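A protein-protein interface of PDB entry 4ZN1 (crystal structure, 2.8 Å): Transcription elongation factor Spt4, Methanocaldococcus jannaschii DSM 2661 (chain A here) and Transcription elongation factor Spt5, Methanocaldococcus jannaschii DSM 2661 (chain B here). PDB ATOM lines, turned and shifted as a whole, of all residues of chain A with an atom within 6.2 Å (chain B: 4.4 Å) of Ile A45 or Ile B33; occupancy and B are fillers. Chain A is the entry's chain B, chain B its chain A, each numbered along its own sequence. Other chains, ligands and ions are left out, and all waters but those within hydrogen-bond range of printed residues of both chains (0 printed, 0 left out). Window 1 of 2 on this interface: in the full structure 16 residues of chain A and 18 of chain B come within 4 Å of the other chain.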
ATOM      1  N   LEU A  43      26.726 -19.537  11.110  1.00  0.00           N
ATOM      2  CA  LEU A  43      27.173 -20.600  12.034  1.00  0.00           C
ATOM      3  C   LEU A  43      26.703 -20.428  13.468  1.00  0.00           C
ATOM      4  O   LEU A  43      26.944 -19.393  14.064  1.00  0.00           O
ATOM      5  CB  LEU A  43      28.700 -20.684  12.021  1.00  0.00           C
ATOM      6  CG  LEU A  43      29.437 -21.378  13.177  1.00  0.00           C
ATOM      7  CD1 LEU A  43      29.725 -22.834  12.862  1.00  0.00           C
ATOM      8  CD2 LEU A  43      30.730 -20.647  13.473  1.00  0.00           C
ATOM      9  N   LEU A  44      26.083 -21.477  14.006  1.00  0.00           N
ATOM     10  CA  LEU A  44      25.650 -21.548  15.397  1.00  0.00           C
ATOM     11  C   LEU A  44      26.307 -22.749  16.025  1.00  0.00           C
ATOM     12  O   LEU A  44      26.076 -23.880  15.609  1.00  0.00           O
ATOM     13  CB  LEU A  44      24.133 -21.725  15.494  1.00  0.00           C
ATOM     14  CG  LEU A  44      23.378 -21.281  16.762  1.00  0.00           C
ATOM     15  CD1 LEU A  44      22.215 -22.221  17.008  1.00  0.00           C
ATOM     16  CD2 LEU A  44      24.213 -21.170  18.023  1.00  0.00           C
ATOM     17  N   ILE A  45      27.134 -22.501  17.029  1.00  0.00           N
ATOM     18  CA  ILE A  45      27.830 -23.561  17.728  1.00  0.00           C
ATOM     19  C   ILE A  45      27.129 -23.688  19.047  1.00  0.00           C
ATOM     20  O   ILE A  45      27.087 -22.722  19.795  1.00  0.00           O
ATOM     21  CB  ILE A  45      29.303 -23.225  17.964  1.00  0.00           C
ATOM     22  CG1 ILE A  45      30.004 -23.083  16.620  1.00  0.00           C
ATOM     23  CG2 ILE A  45      29.954 -24.339  18.774  1.00  0.00           C
ATOM     24  CD1 ILE A  45      31.429 -22.614  16.725  1.00  0.00           C
ATOM     25  N   VAL A  46      26.564 -24.863  19.305  1.00  0.00           N
ATOM     26  CA  VAL A  46      25.861 -25.133  20.548  1.00  0.00           C
ATOM     27  C   VAL A  46      26.761 -26.007  21.417  1.00  0.00           C
ATOM     28  O   VAL A  46      26.943 -27.201  21.138  1.00  0.00           O
ATOM     29  CB  VAL A  46      24.500 -25.821  20.305  1.00  0.00           C
ATOM     30  CG1 VAL A  46      23.755 -26.046  21.617  1.00  0.00           C
ATOM     31  CG2 VAL A  46      23.639 -24.983  19.379  1.00  0.00           C
ATOM     32  N   ILE A  47      27.298 -25.399  22.476  1.00  0.00           N
ATOM     33  CA  ILE A  47      28.198 -26.075  23.400  1.00  0.00           C
ATOM     34  C   ILE A  47      27.373 -26.847  24.439  1.00  0.00           C
ATOM     35  O   ILE A  47      27.768 -27.921  24.867  1.00  0.00           O
ATOM     36  CB  ILE A  47      29.129 -25.106  24.175  1.00  0.00           C
ATOM     37  CG1 ILE A  47      29.593 -23.885  23.349  1.00  0.00           C
ATOM     38  CG2 ILE A  47      30.338 -25.868  24.729  1.00  0.00           C
ATOM     39  CD1 ILE A  47      30.682 -24.159  22.337  1.00  0.00           C
ATOM     40  N   ILE A  54      19.357 -19.589  23.340  1.00  0.00           N
ATOM     41  CA  ILE A  54      19.467 -19.511  21.871  1.00  0.00           C
ATOM     42  C   ILE A  54      19.144 -20.869  21.222  1.00  0.00           C
ATOM     43  O   ILE A  54      18.367 -20.929  20.272  1.00  0.00           O
ATOM     44  CB  ILE A  54      20.873 -19.008  21.419  1.00  0.00           C
ATOM     45  CG1 ILE A  54      21.098 -17.548  21.863  1.00  0.00           C
ATOM     46  CG2 ILE A  54      21.050 -19.119  19.903  1.00  0.00           C
ATOM     47  CD1 ILE A  54      22.487 -16.999  21.575  1.00  0.00           C
ATOM     48  N   GLY A  64      26.537 -29.296  19.019  1.00  0.00           N
ATOM     49  CA  GLY A  64      27.297 -29.353  17.791  1.00  0.00           C
ATOM     50  C   GLY A  64      27.213 -28.071  17.012  1.00  0.00           C
ATOM     51  O   GLY A  64      26.489 -27.146  17.377  1.00  0.00           O
ATOM     52  N   LYS A  65      27.974 -28.042  15.925  1.00  0.00           N
ATOM     53  CA  LYS A  65      28.026 -26.913  15.021  1.00  0.00           C
ATOM     54  C   LYS A  65      26.850 -27.023  14.062  1.00  0.00           C
ATOM     55  O   LYS A  65      26.463 -28.127  13.679  1.00  0.00           O
ATOM     56  CB  LYS A  65      29.342 -26.925  14.243  1.00  0.00           C
ATOM     57  CG  LYS A  65      30.586 -27.011  15.115  1.00  0.00           C
ATOM     58  CD  LYS A  65      31.830 -26.597  14.343  1.00  0.00           C
ATOM     59  CE  LYS A  65      33.094 -26.762  15.180  1.00  0.00           C
ATOM     60  NZ  LYS A  65      33.787 -28.060  14.915  1.00  0.00           N
ATOM     61  N   TYR A  66      26.284 -25.878  13.686  1.00  0.00           N
ATOM     62  CA  TYR A  66      25.115 -25.823  12.806  1.00  0.00           C
ATOM     63  C   TYR A  66      25.231 -24.645  11.863  1.00  0.00           C
ATOM     64  O   TYR A  66      25.640 -23.574  12.282  1.00  0.00           O
ATOM     65  CB  TYR A  66      23.838 -25.645  13.625  1.00  0.00           C
ATOM     66  CG  TYR A  66      23.408 -26.862  14.404  1.00  0.00           C
ATOM     67  CD1 TYR A  66      22.669 -27.872  13.796  1.00  0.00           C
ATOM     68  CD2 TYR A  66      23.724 -26.997  15.752  1.00  0.00           C
ATOM     69  CE1 TYR A  66      22.268 -28.992  14.507  1.00  0.00           C
ATOM     70  CE2 TYR A  66      23.324 -28.109  16.473  1.00  0.00           C
ATOM     71  CZ  TYR A  66      22.600 -29.104  15.850  1.00  0.00           C
ATOM     72  OH  TYR A  66      22.215 -30.195  16.581  1.00  0.00           O
ATOM     73  N   ALA B  16      34.992 -18.079  16.387  1.00  0.00           N
ATOM     74  CA  ALA B  16      33.936 -18.886  17.025  1.00  0.00           C
ATOM     75  C   ALA B  16      34.425 -20.312  17.265  1.00  0.00           C
ATOM     76  O   ALA B  16      34.340 -20.823  18.382  1.00  0.00           O
ATOM     77  CB  ALA B  16      32.666 -18.892  16.183  1.00  0.00           C
ATOM     78  N   GLY B  17      34.978 -20.922  16.215  1.00  0.00           N
ATOM     79  CA  GLY B  17      35.531 -22.282  16.275  1.00  0.00           C
ATOM     80  C   GLY B  17      36.505 -22.520  17.415  1.00  0.00           C
ATOM     81  O   GLY B  17      36.401 -23.519  18.125  1.00  0.00           O
ATOM     82  N   MET B  19      36.774 -20.466  20.032  1.00  0.00           N
ATOM     83  CA  MET B  19      36.028 -20.100  21.245  1.00  0.00           C
ATOM     84  C   MET B  19      35.339 -21.326  21.810  1.00  0.00           C
ATOM     85  O   MET B  19      35.388 -21.595  23.010  1.00  0.00           O
ATOM     86  CB  MET B  19      34.976 -19.017  20.947  1.00  0.00           C
ATOM     87  CG  MET B  19      35.361 -17.617  21.389  1.00  0.00           C
ATOM     88  SD  MET B  19      34.470 -16.243  20.602  1.00  0.00           S
ATOM     89  CE  MET B  19      32.798 -16.834  20.615  1.00  0.00           C
ATOM     90  N   ALA B  20      34.688 -22.065  20.923  1.00  0.00           N
ATOM     91  CA  ALA B  20      34.101 -23.347  21.283  1.00  0.00           C
ATOM     92  C   ALA B  20      35.146 -24.278  21.910  1.00  0.00           C
ATOM     93  O   ALA B  20      34.895 -24.882  22.947  1.00  0.00           O
ATOM     94  CB  ALA B  20      33.460 -23.996  20.062  1.00  0.00           C
ATOM     95  N   VAL B  30      30.338 -21.303  28.751  1.00  0.00           N
ATOM     96  CA  VAL B  30      29.929 -20.745  27.454  1.00  0.00           C
ATOM     97  C   VAL B  30      28.991 -21.763  26.818  1.00  0.00           C
ATOM     98  O   VAL B  30      29.359 -22.922  26.634  1.00  0.00           O
ATOM     99  CB  VAL B  30      31.148 -20.529  26.527  1.00  0.00           C
ATOM    100  CG1 VAL B  30      30.723 -20.054  25.140  1.00  0.00           C
ATOM    101  CG2 VAL B  30      32.113 -19.528  27.142  1.00  0.00           C
ATOM    102  N   SER B  32      26.396 -21.181  23.958  1.00  0.00           N
ATOM    103  CA  SER B  32      26.299 -21.161  22.509  1.00  0.00           C
ATOM    104  C   SER B  32      27.105 -20.004  21.944  1.00  0.00           C
ATOM    105  O   SER B  32      27.395 -19.027  22.633  1.00  0.00           O
ATOM    106  CB  SER B  32      24.845 -21.067  22.057  1.00  0.00           C
ATOM    107  OG  SER B  32      24.490 -19.727  21.802  1.00  0.00           O
ATOM    108  N   ILE B  33      27.486 -20.137  20.685  1.00  0.00           N
ATOM    109  CA  ILE B  33      28.187 -19.078  19.989  1.00  0.00           C
ATOM    110  C   ILE B  33      27.552 -18.933  18.627  1.00  0.00           C
ATOM    111  O   ILE B  33      27.291 -19.936  17.963  1.00  0.00           O
ATOM    112  CB  ILE B  33      29.666 -19.411  19.837  1.00  0.00           C
ATOM    113  CG1 ILE B  33      30.316 -19.578  21.220  1.00  0.00           C
ATOM    114  CG2 ILE B  33      30.367 -18.334  19.008  1.00  0.00           C
ATOM    115  CD1 ILE B  33      31.594 -20.379  21.173  1.00  0.00           C
ATOM    116  N   LEU B  34      27.328 -17.686  18.220  1.00  0.00           N
ATOM    117  CA  LEU B  34      26.614 -17.373  16.993  1.00  0.00           C
ATOM    118  C   LEU B  34      27.404 -16.417  16.086  1.00  0.00           C
ATOM    119  O   LEU B  34      27.835 -15.350  16.518  1.00  0.00           O
ATOM    120  CB  LEU B  34      25.263 -16.772  17.343  1.00  0.00           C
ATOM    121  CG  LEU B  34      24.324 -16.460  16.182  1.00  0.00           C
ATOM    122  CD1 LEU B  34      24.019 -17.684  15.342  1.00  0.00           C
ATOM    123  CD2 LEU B  34      23.036 -15.897  16.741  1.00  0.00           C
ATOM    124  N   ALA B  35      27.586 -16.826  14.828  1.00  0.00           N
ATOM    125  CA  ALA B  35      28.251 -16.026  13.814  1.00  0.00           C
ATOM    126  C   ALA B  35      27.335 -15.982  12.607  1.00  0.00           C
ATOM    127  O   ALA B  35      27.142 -16.999  11.939  1.00  0.00           O
ATOM    128  CB  ALA B  35      29.587 -16.645  13.450  1.00  0.00           C
ATOM    129  N   VAL B  43      30.953 -11.644  16.799  1.00  0.00           N
ATOM    130  CA  VAL B  43      30.583 -13.005  17.122  1.00  0.00           C
ATOM    131  C   VAL B  43      29.796 -12.904  18.409  1.00  0.00           C
ATOM    132  O   VAL B  43      30.305 -12.414  19.398  1.00  0.00           O
ATOM    133  CB  VAL B  43      31.820 -13.879  17.327  1.00  0.00           C
ATOM    134  CG1 VAL B  43      31.404 -15.295  17.675  1.00  0.00           C
ATOM    135  CG2 VAL B  43      32.672 -13.905  16.067  1.00  0.00           C
ATOM    136  N   LEU B  44      28.551 -13.346  18.394  1.00  0.00           N
ATOM    137  CA  LEU B  44      27.740 -13.365  19.603  1.00  0.00           C
ATOM    138  C   LEU B  44      28.064 -14.606  20.400  1.00  0.00           C
ATOM    139  O   LEU B  44      28.099 -15.714  19.864  1.00  0.00           O
ATOM    140  CB  LEU B  44      26.250 -13.339  19.291  1.00  0.00           C
ATOM    141  CG  LEU B  44      25.839 -12.142  18.441  1.00  0.00           C
ATOM    142  CD1 LEU B  44      24.339 -12.198  18.245  1.00  0.00           C
ATOM    143  CD2 LEU B  44      26.268 -10.820  19.054  1.00  0.00           C
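Of chain B, only Ala B16 (3.8 Å), Gly B17 (3.96 Å), Ala B20 (3.8 Å), Ser B32 (3.2 Å) and Ile B33 (2.7 Å) come within 4 Å of Ile A45. Ile B33 touches three residues of chain A. Of the printed residues of chain A, Ser B32 touches Ile A45 and Ile A54. Printed residues of chain B within 4 Å of Leu A44: Ile B33 and Leu B34. Printed residues of chain A within 4 Å of Ala B16: Leu A43 (3.8 Å) and Ile A45 (3.8 Å). Of the printed residues of chain A, Ala B20 touches Ile A45 (3.8 Å) and Ile A47 (3.6 Å). Gly A64 touches none of the printed residues of chain B.
The backbone carbonyl oxygen of Leu B44 sits at hydrogen-bond distance from the backbone NH of Leu B34 (2.7 Å). The backbone NH of Leu A44 sits at hydrogen-bond distance from the backbone carbonyl oxygen of Tyr A66 (2.8 Å).
The backbone carbonyl oxygen of Ile B33 is in hydrogen-bond range of the backbone NH of Ile A45 (2.7 Å). O of Ala B35 lies within hydrogen-bond range of N of Leu A43, 2.7 Å away.
Among the printed residues, pairs that only touch across the chains: Leu A43 with Ala B16 (3.8 Å), Leu A43 with Ile B33 (3.95 Å), Leu A43 with Leu B34 (3.6 Å), Leu A44 with Ile B33 (3.3 Å), Leu A44 with Leu B34 (3.9 Å), Ile A45 with Ala B16 (3.8 Å), Ile A45 with Gly B17 (3.96 Å), Ile A45 with Ala B20 (3.8 Å), Ile A45 with Ser B32 (3.2 Å), Ile A47 with Ala B20 (3.6 Å), Ile A47 with Val B30 (3.3 Å) and Ile A54 with Ser B32 (3.4 Å).
Of the 9 printed residues of chain A, 5 touch a printed residue of chain B. Hydrophobic or aromatic side chains of chain A that line the printed part of chain B: Leu A43, Leu A44, Ile A45, Ile A47 and Ile A54. Among the printed residues, 14 pairs touch across the chains. Among the printed residues, no Asp or Glu carboxylate lies within 4 Å of a Lys or Arg side-chain nitrogen of the other chain.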
